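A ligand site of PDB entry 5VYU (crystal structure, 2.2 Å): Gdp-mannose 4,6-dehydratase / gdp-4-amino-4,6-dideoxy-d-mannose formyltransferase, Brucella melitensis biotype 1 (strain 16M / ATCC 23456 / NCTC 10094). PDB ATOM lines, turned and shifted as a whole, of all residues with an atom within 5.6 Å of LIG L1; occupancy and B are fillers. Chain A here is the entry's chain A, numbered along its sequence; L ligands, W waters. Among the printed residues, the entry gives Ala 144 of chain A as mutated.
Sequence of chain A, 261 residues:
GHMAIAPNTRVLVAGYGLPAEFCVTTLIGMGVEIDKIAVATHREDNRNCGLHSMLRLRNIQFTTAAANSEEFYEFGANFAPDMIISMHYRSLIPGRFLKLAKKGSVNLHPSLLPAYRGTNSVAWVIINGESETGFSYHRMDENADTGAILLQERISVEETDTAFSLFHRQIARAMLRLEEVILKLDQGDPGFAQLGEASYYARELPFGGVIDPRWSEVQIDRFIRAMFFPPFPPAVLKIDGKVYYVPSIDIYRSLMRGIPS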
ATOM      1  N   SER A  86      -8.221 -12.524   3.465  1.00  0.00           N
ATOM      2  CA  SER A  86      -8.578 -12.307   4.866  1.00  0.00           C
ATOM      3  C   SER A  86     -10.079 -12.281   4.962  1.00  0.00           C
ATOM      4  O   SER A  86     -10.719 -11.470   4.295  1.00  0.00           O
ATOM      5  CB  SER A  86      -8.023 -11.019   5.394  1.00  0.00           C
ATOM      6  OG  SER A  86      -8.697 -10.699   6.595  1.00  0.00           O
ATOM      7  N   TYR A  89     -10.434 -12.211   9.653  1.00  0.00           N
ATOM      8  CA  TYR A  89      -9.221 -12.349  10.438  1.00  0.00           C
ATOM      9  C   TYR A  89      -9.177 -11.184  11.437  1.00  0.00           C
ATOM     10  O   TYR A  89      -9.500 -10.030  11.084  1.00  0.00           O
ATOM     11  CB  TYR A  89      -7.989 -12.375   9.514  1.00  0.00           C
ATOM     12  CG  TYR A  89      -6.759 -12.919  10.213  1.00  0.00           C
ATOM     13  CD1 TYR A  89      -6.693 -14.245  10.568  1.00  0.00           C
ATOM     14  CD2 TYR A  89      -5.694 -12.097  10.553  1.00  0.00           C
ATOM     15  CE1 TYR A  89      -5.584 -14.777  11.216  1.00  0.00           C
ATOM     16  CE2 TYR A  89      -4.564 -12.611  11.205  1.00  0.00           C
ATOM     17  CZ  TYR A  89      -4.525 -13.954  11.535  1.00  0.00           C
ATOM     18  OH  TYR A  89      -3.459 -14.491  12.182  1.00  0.00           O
ATOM     19  N   ARG A  90      -8.749 -11.485  12.648  1.00  0.00           N
ATOM     20  CA  ARG A  90      -8.933 -10.608  13.825  1.00  0.00           C
ATOM     21  C   ARG A  90      -7.665  -9.945  14.330  1.00  0.00           C
ATOM     22  O   ARG A  90      -7.674  -9.390  15.433  1.00  0.00           O
ATOM     23  CB  ARG A  90      -9.572 -11.405  14.960  1.00  0.00           C
ATOM     24  CG  ARG A  90     -11.008 -11.895  14.642  1.00  0.00           C
ATOM     25  CD  ARG A  90     -11.591 -12.705  15.786  1.00  0.00           C
ATOM     26  NE  ARG A  90     -12.147 -11.816  16.813  1.00  0.00           N
ATOM     27  CZ  ARG A  90     -13.344 -11.185  16.767  1.00  0.00           C
ATOM     28  NH1 ARG A  90     -14.183 -11.323  15.738  1.00  0.00           N
ATOM     29  NH2 ARG A  90     -13.679 -10.384  17.789  1.00  0.00           N
ATOM     30  N   SER A  91      -6.592  -9.973  13.531  1.00  0.00           N
ATOM     31  CA  SER A  91      -5.334  -9.299  13.838  1.00  0.00           C
ATOM     32  C   SER A  91      -4.867  -8.534  12.618  1.00  0.00           C
ATOM     33  O   SER A  91      -5.298  -8.823  11.507  1.00  0.00           O
ATOM     34  CB  SER A  91      -4.260 -10.308  14.191  1.00  0.00           C
ATOM     35  OG  SER A  91      -4.705 -11.180  15.203  1.00  0.00           O
ATOM     36  N   LEU A  92      -3.999  -7.548  12.844  1.00  0.00           N
ATOM     37  CA  LEU A  92      -3.323  -6.862  11.751  1.00  0.00           C
ATOM     38  C   LEU A  92      -2.262  -7.782  11.198  1.00  0.00           C
ATOM     39  O   LEU A  92      -1.469  -8.339  11.972  1.00  0.00           O
ATOM     40  CB  LEU A  92      -2.644  -5.599  12.271  1.00  0.00           C
ATOM     41  CG  LEU A  92      -2.164  -4.625  11.213  1.00  0.00           C
ATOM     42  CD1 LEU A  92      -3.312  -3.840  10.600  1.00  0.00           C
ATOM     43  CD2 LEU A  92      -1.167  -3.680  11.884  1.00  0.00           C
ATOM     44  N   ILE A  93      -2.234  -7.968   9.889  1.00  0.00           N
ATOM     45  CA  ILE A  93      -1.253  -8.858   9.284  1.00  0.00           C
ATOM     46  C   ILE A  93      -0.027  -8.048   8.891  1.00  0.00           C
ATOM     47  O   ILE A  93      -0.140  -7.058   8.222  1.00  0.00           O
ATOM     48  CB  ILE A  93      -1.819  -9.589   8.066  1.00  0.00           C
ATOM     49  CG1 ILE A  93      -3.008 -10.442   8.505  1.00  0.00           C
ATOM     50  CG2 ILE A  93      -0.728 -10.463   7.446  1.00  0.00           C
ATOM     51  CD1 ILE A  93      -4.088 -10.530   7.451  1.00  0.00           C
ATOM     52  N   PRO A  94       1.146  -8.472   9.353  1.00  0.00           N
ATOM     53  CA  PRO A  94       2.338  -7.635   9.124  1.00  0.00           C
ATOM     54  C   PRO A  94       2.689  -7.574   7.666  1.00  0.00           C
ATOM     55  O   PRO A  94       2.414  -8.520   6.891  1.00  0.00           O
ATOM     56  CB  PRO A  94       3.449  -8.296   9.936  1.00  0.00           C
ATOM     57  CG  PRO A  94       2.901  -9.586  10.406  1.00  0.00           C
ATOM     58  CD  PRO A  94       1.406  -9.574  10.283  1.00  0.00           C
ATOM     59  N   LEU A  98       2.305 -10.189   4.087  1.00  0.00           N
ATOM     60  CA  LEU A  98       1.581  -9.877   2.870  1.00  0.00           C
ATOM     61  C   LEU A  98       2.488  -9.900   1.640  1.00  0.00           C
ATOM     62  O   LEU A  98       2.182 -10.414   0.605  1.00  0.00           O
ATOM     63  CB  LEU A  98       0.961  -8.478   2.999  1.00  0.00           C
ATOM     64  CG  LEU A  98      -0.124  -8.305   4.075  1.00  0.00           C
ATOM     65  CD1 LEU A  98      -0.387  -6.812   4.353  1.00  0.00           C
ATOM     66  CD2 LEU A  98      -1.382  -9.069   3.663  1.00  0.00           C
ATOM     67  N   ASN A 107      -9.252  -8.323   1.776  1.00  0.00           N
ATOM     68  CA  ASN A 107      -9.924  -8.412   3.042  1.00  0.00           C
ATOM     69  C   ASN A 107     -11.338  -7.994   2.814  1.00  0.00           C
ATOM     70  O   ASN A 107     -11.588  -7.097   1.998  1.00  0.00           O
ATOM     71  CB  ASN A 107      -9.251  -7.456   4.021  1.00  0.00           C
ATOM     72  CG  ASN A 107      -9.991  -7.347   5.322  1.00  0.00           C
ATOM     73  OD1 ASN A 107     -10.629  -6.340   5.594  1.00  0.00           O
ATOM     74  ND2 ASN A 107      -9.900  -8.329   6.126  1.00  0.00           N
ATOM     75  N   LEU A 108     -12.246  -8.632   3.537  1.00  0.00           N
ATOM     76  CA  LEU A 108     -13.646  -8.225   3.591  1.00  0.00           C
ATOM     77  C   LEU A 108     -13.918  -7.264   4.764  1.00  0.00           C
ATOM     78  O   LEU A 108     -13.795  -7.645   5.929  1.00  0.00           O
ATOM     79  CB  LEU A 108     -14.532  -9.457   3.720  1.00  0.00           C
ATOM     80  CG  LEU A 108     -16.023  -9.202   4.004  1.00  0.00           C
ATOM     81  CD1 LEU A 108     -16.680  -8.216   3.035  1.00  0.00           C
ATOM     82  CD2 LEU A 108     -16.750 -10.552   3.995  1.00  0.00           C
ATOM     83  N   HIS A 109     -14.360  -6.058   4.472  1.00  0.00           N
ATOM     84  CA  HIS A 109     -14.733  -5.115   5.520  1.00  0.00           C
ATOM     85  C   HIS A 109     -16.172  -4.708   5.379  1.00  0.00           C
ATOM     86  O   HIS A 109     -16.567  -4.294   4.288  1.00  0.00           O
ATOM     87  CB  HIS A 109     -13.875  -3.874   5.503  1.00  0.00           C
ATOM     88  CG  HIS A 109     -14.066  -3.054   6.721  1.00  0.00           C
ATOM     89  ND1 HIS A 109     -13.520  -3.400   7.939  1.00  0.00           N
ATOM     90  CD2 HIS A 109     -14.855  -1.979   6.950  1.00  0.00           C
ATOM     91  CE1 HIS A 109     -13.932  -2.537   8.853  1.00  0.00           C
ATOM     92  NE2 HIS A 109     -14.746  -1.672   8.276  1.00  0.00           N
ATOM     93  N   HIS A 138     -11.225  -5.221  -0.186  1.00  0.00           N
ATOM     94  CA  HIS A 138     -10.086  -4.378  -0.553  1.00  0.00           C
ATOM     95  C   HIS A 138      -8.747  -5.044  -0.320  1.00  0.00           C
ATOM     96  O   HIS A 138      -8.604  -5.892   0.562  1.00  0.00           O
ATOM     97  CB  HIS A 138     -10.105  -3.106   0.253  1.00  0.00           C
ATOM     98  CG  HIS A 138      -9.928  -3.345   1.707  1.00  0.00           C
ATOM     99  ND1 HIS A 138      -8.694  -3.380   2.304  1.00  0.00           N
ATOM    100  CD2 HIS A 138     -10.834  -3.625   2.675  1.00  0.00           C
ATOM    101  CE1 HIS A 138      -8.841  -3.650   3.590  1.00  0.00           C
ATOM    102  NE2 HIS A 138     -10.131  -3.799   3.838  1.00  0.00           N
ATOM    103  N   ARG A 139      -7.741  -4.579  -1.048  1.00  0.00           N
ATOM    104  CA  ARG A 139      -6.389  -5.140  -0.901  1.00  0.00           C
ATOM    105  C   ARG A 139      -5.888  -4.677   0.417  1.00  0.00           C
ATOM    106  O   ARG A 139      -6.245  -3.571   0.828  1.00  0.00           O
ATOM    107  CB  ARG A 139      -5.477  -4.665  -2.031  1.00  0.00           C
ATOM    108  CG  ARG A 139      -5.882  -5.163  -3.415  1.00  0.00           C
ATOM    109  CD  ARG A 139      -4.949  -4.632  -4.505  1.00  0.00           C
ATOM    110  NE  ARG A 139      -5.071  -5.402  -5.748  1.00  0.00           N
ATOM    111  CZ  ARG A 139      -4.515  -6.602  -5.965  1.00  0.00           C
ATOM    112  NH1 ARG A 139      -4.711  -7.200  -7.125  1.00  0.00           N
ATOM    113  NH2 ARG A 139      -3.774  -7.212  -5.024  1.00  0.00           N
ATOM    114  N   MET A 140      -5.098  -5.514   1.092  1.00  0.00           N
ATOM    115  CA  MET A 140      -4.506  -5.150   2.355  1.00  0.00           C
ATOM    116  C   MET A 140      -3.137  -4.518   2.136  1.00  0.00           C
ATOM    117  O   MET A 140      -2.243  -5.127   1.549  1.00  0.00           O
ATOM    118  CB  MET A 140      -4.406  -6.353   3.300  1.00  0.00           C
ATOM    119  CG  MET A 140      -5.773  -6.851   3.773  1.00  0.00           C
ATOM    120  SD  MET A 140      -5.565  -8.229   4.916  1.00  0.00           S
ATOM    121  CE  MET A 140      -5.045  -9.547   3.795  1.00  0.00           C
ATOM    122  N   ASP A 141      -2.997  -3.287   2.607  1.00  0.00           N
ATOM    123  CA  ASP A 141      -1.666  -2.721   2.798  1.00  0.00           C
ATOM    124  C   ASP A 141      -1.332  -2.824   4.298  1.00  0.00           C
ATOM    125  O   ASP A 141      -2.054  -3.459   5.047  1.00  0.00           O
ATOM    126  CB  ASP A 141      -1.558  -1.309   2.207  1.00  0.00           C
ATOM    127  CG  ASP A 141      -2.455  -0.350   2.852  1.00  0.00           C
ATOM    128  OD1 ASP A 141      -2.638  -0.494   4.069  1.00  0.00           O
ATOM    129  OD2 ASP A 141      -2.991   0.531   2.157  1.00  0.00           O
ATOM    130  N   GLU A 142      -0.247  -2.230   4.747  1.00  0.00           N
ATOM    131  CA  GLU A 142       0.232  -2.553   6.086  1.00  0.00           C
ATOM    132  C   GLU A 142      -0.587  -1.907   7.220  1.00  0.00           C
ATOM    133  O   GLU A 142      -0.536  -2.385   8.349  1.00  0.00           O
ATOM    134  CB  GLU A 142       1.740  -2.322   6.208  1.00  0.00           C
ATOM    135  CG  GLU A 142       2.149  -0.886   6.351  1.00  0.00           C
ATOM    136  CD  GLU A 142       3.650  -0.742   6.506  1.00  0.00           C
ATOM    137  OE1 GLU A 142       4.293  -1.664   7.103  1.00  0.00           O
ATOM    138  OE2 GLU A 142       4.153   0.310   6.038  1.00  0.00           O
ATOM    139  N   ASN A 143      -1.361  -0.862   6.889  1.00  0.00           N
ATOM    140  CA  ASN A 143      -2.412  -0.330   7.772  1.00  0.00           C
ATOM    141  C   ASN A 143      -3.768  -0.970   7.494  1.00  0.00           C
ATOM    142  O   ASN A 143      -3.987  -1.591   6.462  1.00  0.00           O
ATOM    143  CB  ASN A 143      -2.526   1.187   7.624  1.00  0.00           C
ATOM    144  CG  ASN A 143      -1.207   1.908   7.892  1.00  0.00           C
ATOM    145  OD1 ASN A 143      -0.209   1.287   8.277  1.00  0.00           O
ATOM    146  ND2 ASN A 143      -1.186   3.220   7.683  1.00  0.00           N
ATOM    147  N   ALA A 144      -4.689  -0.785   8.425  1.00  0.00           N
ATOM    148  CA  ALA A 144      -5.940  -1.498   8.409  1.00  0.00           C
ATOM    149  C   ALA A 144      -6.974  -0.774   7.549  1.00  0.00           C
ATOM    150  O   ALA A 144      -7.172   0.433   7.702  1.00  0.00           O
ATOM    151  CB  ALA A 144      -6.433  -1.660   9.839  1.00  0.00           C
ATOM    152  N   ASP A 145      -7.598  -1.486   6.619  1.00  0.00           N
ATOM    153  CA  ASP A 145      -8.759  -0.976   5.901  1.00  0.00           C
ATOM    154  C   ASP A 145      -8.480   0.216   4.959  1.00  0.00           C
ATOM    155  O   ASP A 145      -9.397   0.941   4.574  1.00  0.00           O
ATOM    156  CB  ASP A 145      -9.892  -0.650   6.903  1.00  0.00           C
ATOM    157  CG  ASP A 145     -10.165  -1.786   7.867  1.00  0.00           C
ATOM    158  OD1 ASP A 145      -9.983  -2.981   7.494  1.00  0.00           O
ATOM    159  OD2 ASP A 145     -10.566  -1.491   8.999  1.00  0.00           O
ATOM    160  N   THR A 146      -7.223   0.402   4.573  1.00  0.00           N
ATOM    161  CA  THR A 146      -6.823   1.555   3.750  1.00  0.00           C
ATOM    162  C   THR A 146      -6.518   1.197   2.304  1.00  0.00           C
ATOM    163  O   THR A 146      -6.457   2.086   1.442  1.00  0.00           O
ATOM    164  CB  THR A 146      -5.568   2.172   4.340  1.00  0.00           C
ATOM    165  OG1 THR A 146      -4.676   1.120   4.714  1.00  0.00           O
ATOM    166  CG2 THR A 146      -5.906   3.012   5.558  1.00  0.00           C
ATOM    167  N   GLY A 147      -6.376  -0.104   2.027  1.00  0.00           N
ATOM    168  CA  GLY A 147      -5.906  -0.548   0.730  1.00  0.00           C
ATOM    169  C   GLY A 147      -6.956  -0.455  -0.344  1.00  0.00           C
ATOM    170  O   GLY A 147      -8.098  -0.242  -0.055  1.00  0.00           O
HETATM  171  N1  LIG L   1      -4.067  -6.413   8.122  1.00  0.00           N
HETATM  172  C1  LIG L   1      -3.546  -5.458   7.331  1.00  0.00           C
HETATM  173  N2  LIG L   1      -2.245  -5.266   7.289  1.00  0.00           N
HETATM  174  N3  LIG L   1      -4.356  -4.654   6.557  1.00  0.00           N
HETATM  175  C2  LIG L   1      -5.712  -4.773   6.565  1.00  0.00           C
HETATM  176  O1  LIG L   1      -6.402  -4.041   5.865  1.00  0.00           O
HETATM  177  C3  LIG L   1      -6.274  -5.819   7.385  1.00  0.00           C
HETATM  178  N4  LIG L   1      -7.640  -5.981   7.491  1.00  0.00           N
HETATM  179  C4  LIG L   1      -8.129  -6.586   8.720  1.00  0.00           C
HETATM  180  C5  LIG L   1      -7.335  -7.854   9.029  1.00  0.00           C
HETATM  181  N5  LIG L   1      -5.901  -7.575   8.985  1.00  0.00           N
HETATM  182  C6  LIG L   1      -5.395  -6.613   8.143  1.00  0.00           C
HETATM  183  C7  LIG L   1      -8.036  -5.587   9.894  1.00  0.00           C
HETATM  184  N6  LIG L   1      -8.535  -6.130  11.200  1.00  0.00           N
HETATM  185  C8  LIG L   1      -6.236  -5.144  14.678  1.00  0.00           C
HETATM  186  C9  LIG L   1      -6.340  -4.260  13.623  1.00  0.00           C
HETATM  187  C10 LIG L   1      -7.070  -4.586  12.490  1.00  0.00           C
HETATM  188  C11 LIG L   1      -7.720  -5.824  12.366  1.00  0.00           C
HETATM  189  C12 LIG L   1      -7.632  -6.705  13.441  1.00  0.00           C
HETATM  190  C13 LIG L   1      -6.906  -6.367  14.595  1.00  0.00           C
HETATM  191  C14 LIG L   1      -5.433  -4.749  15.916  1.00  0.00           C
HETATM  192  N7  LIG L   1      -5.040  -3.469  15.992  1.00  0.00           N
HETATM  193  C15 LIG L   1      -9.732  -6.783  11.228  1.00  0.00           C
HETATM  194  O2  LIG L   1     -10.663  -6.700  10.365  1.00  0.00           O
HETATM  195  O3  LIG L   1      -5.180  -5.566  16.817  1.00  0.00           O
HETATM  196  O1  LG2 L   2     -19.859  -6.024  23.844  1.00  0.00           O
HETATM  197  C1  LG2 L   2     -20.728  -5.980  22.973  1.00  0.00           C
HETATM  198  C2  LG2 L   2     -20.343  -6.306  21.655  1.00  0.00           C
HETATM  199  N1  LG2 L   2     -19.162  -6.687  21.103  1.00  0.00           N
HETATM  200  C3  LG2 L   2     -19.388  -6.866  19.785  1.00  0.00           C
HETATM  201  N2  LG2 L   2     -22.007  -5.611  23.245  1.00  0.00           N
HETATM  202  C4  LG2 L   2     -22.938  -5.553  22.245  1.00  0.00           C
HETATM  203  N3  LG2 L   2     -24.190  -5.185  22.532  1.00  0.00           N
HETATM  204  N4  LG2 L   2     -22.610  -5.881  20.944  1.00  0.00           N
HETATM  205  C5  LG2 L   2     -21.320  -6.257  20.640  1.00  0.00           C
HETATM  206  N5  LG2 L   2     -20.685  -6.614  19.514  1.00  0.00           N
HETATM  207  C6  LG2 L   2     -21.326  -6.685  18.155  1.00  0.00           C
HETATM  208  O2  LG2 L   2     -20.868  -7.798  17.364  1.00  0.00           O
HETATM  209  C7  LG2 L   2     -21.011  -5.429  17.338  1.00  0.00           C
HETATM  210  O3  LG2 L   2     -22.266  -4.931  16.888  1.00  0.00           O
HETATM  211  C8  LG2 L   2     -20.066  -5.883  16.220  1.00  0.00           C
HETATM  212  O4  LG2 L   2     -20.170  -5.198  14.944  1.00  0.00           O
HETATM  213  C9  LG2 L   2     -20.441  -7.351  16.083  1.00  0.00           C
HETATM  214  C10 LG2 L   2     -19.306  -8.231  15.604  1.00  0.00           C
HETATM  215  O5  LG2 L   2     -18.238  -8.185  16.550  1.00  0.00           O
HETATM  216  P1  LG2 L   2     -16.749  -8.498  16.085  1.00  0.00           P
HETATM  217  O6  LG2 L   2     -15.812  -8.225  17.239  1.00  0.00           O
HETATM  218  O7  LG2 L   2     -16.752  -9.937  15.599  1.00  0.00           O
HETATM  219  O8  LG2 L   2     -16.397  -7.528  14.822  1.00  0.00           O
HETATM  220  P2  LG2 L   2     -15.499  -6.178  14.909  1.00  0.00           P
HETATM  221  O9  LG2 L   2     -15.331  -5.654  13.480  1.00  0.00           O
HETATM  222  O10 LG2 L   2     -16.198  -5.039  15.637  1.00  0.00           O
HETATM  223  O11 LG2 L   2     -14.071  -6.460  15.668  1.00  0.00           O
HETATM  224  C11 LG2 L   2     -12.976  -7.326  15.296  1.00  0.00           C
HETATM  225  O12 LG2 L   2     -12.574  -7.027  13.956  1.00  0.00           O
HETATM  226  C12 LG2 L   2     -12.259  -5.623  13.793  1.00  0.00           C
HETATM  227  C13 LG2 L   2     -12.407  -5.210  12.314  1.00  0.00           C
HETATM  228  C14 LG2 L   2     -11.748  -7.156  16.229  1.00  0.00           C
HETATM  229  O13 LG2 L   2     -10.824  -8.233  16.028  1.00  0.00           O
HETATM  230  C15 LG2 L   2     -11.035  -5.800  16.027  1.00  0.00           C
HETATM  231  O14 LG2 L   2      -9.757  -5.783  16.666  1.00  0.00           O
HETATM  232  C16 LG2 L   2     -10.917  -5.401  14.525  1.00  0.00           C
HETATM  233  N6  LG2 L   2     -10.430  -4.014  14.307  1.00  0.00           N
HETATM  234  O   HOH W   1      -5.460  -1.893   3.952  1.00  0.00           O
HETATM  235  O   HOH W   2     -11.611  -5.160   8.479  1.00  0.00           O
HETATM  236  O   HOH W   3      -3.498  -7.380  15.616  1.00  0.00           O
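The backbone NH (N) of Asn 143 lies within hydrogen-bond range of the side-chain carboxylate (OD1) of Asp 141.
The side-chain carboxylate of Asp 141 lies within hydrogen-bond range of the side-chain hydroxyl of Thr 146.
The backbone NH (N) of Gly 147 lies close to the side-chain carboxylate (OD2) of Asp 141 (3.4 Å).
The backbone carbonyl oxygen (O) of Asn 143 is in hydrogen-bond range of the side-chain hydroxyl (OG1) of Thr 146 (3.3 Å).
The backbone carbonyl oxygen (O) of His 138 lies within hydrogen-bond range of the backbone NH (N) of Asn 107.
The side-chain amide nitrogen (ND2) of Asn 107 is in hydrogen-bond range of the side-chain hydroxyl (OG) of Ser 86, 2.7 Å away.
N of Leu 108 lies within hydrogen-bond range of O of Ser 86 (3.3 Å).
OG of Ser 86 touches C5 of LIG L1, at 3.98 Å.
Tyr 89 touches LIG L1.
Arg 90 touches LIG L1.
N of Leu 92 touches C13 of LIG L1 (3.6 Å).
Leu 98 touches LIG L1 (CD1 to N2, 3.8 Å).
Asn 107 touches LIG L1.
CE1 of His 138 touches O1 of LIG L1, at 3.4 Å.
Met 140 touches LIG L1 (CG to C2, 3.5 Å).
O of Glu 142 touches N2 of LIG L1, 3.5 Å away.
Ala 144 touches LIG L1.
Of the 21 residues printed, 15 come within 4 Å of LIG L1.
Water W3 lies within hydrogen-bond range of O3 of LIG L1 (2.7 Å) and N of Leu 92 (2.8 Å).
A nitrogen (N5) of LIG L1 sits at hydrogen-bond distance from the backbone carbonyl oxygen (O) of Ser 91 (2.9 Å).
The backbone carbonyl oxygen of Asp 141 is in hydrogen-bond range of a nitrogen (N2) of LIG L1 (2.9 Å).
A nitrogen (N1) of LIG L1 lies within hydrogen-bond range of the backbone NH (N) of Ile 93 (3.0 Å).
The backbone carbonyl oxygen (O) of Ile 93 lies within hydrogen-bond range of a nitrogen (N2) of LIG L1 (2.9 Å).
The backbone NH (N) of Asp 145 is in hydrogen-bond range of an oxygen (O1) of LIG L1, at 2.9 Å.
O of Asn 143 is in hydrogen-bond range of N3 of LIG L1, 3.1 Å away.
O of Arg 90 is in hydrogen-bond range of O13 of LG2 L2 (3.4 Å).
The guanidinium group (NH1) of Arg 90 lies within salt-bridge range of an oxygen (O7) of LG2 L2 (2.9 Å).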
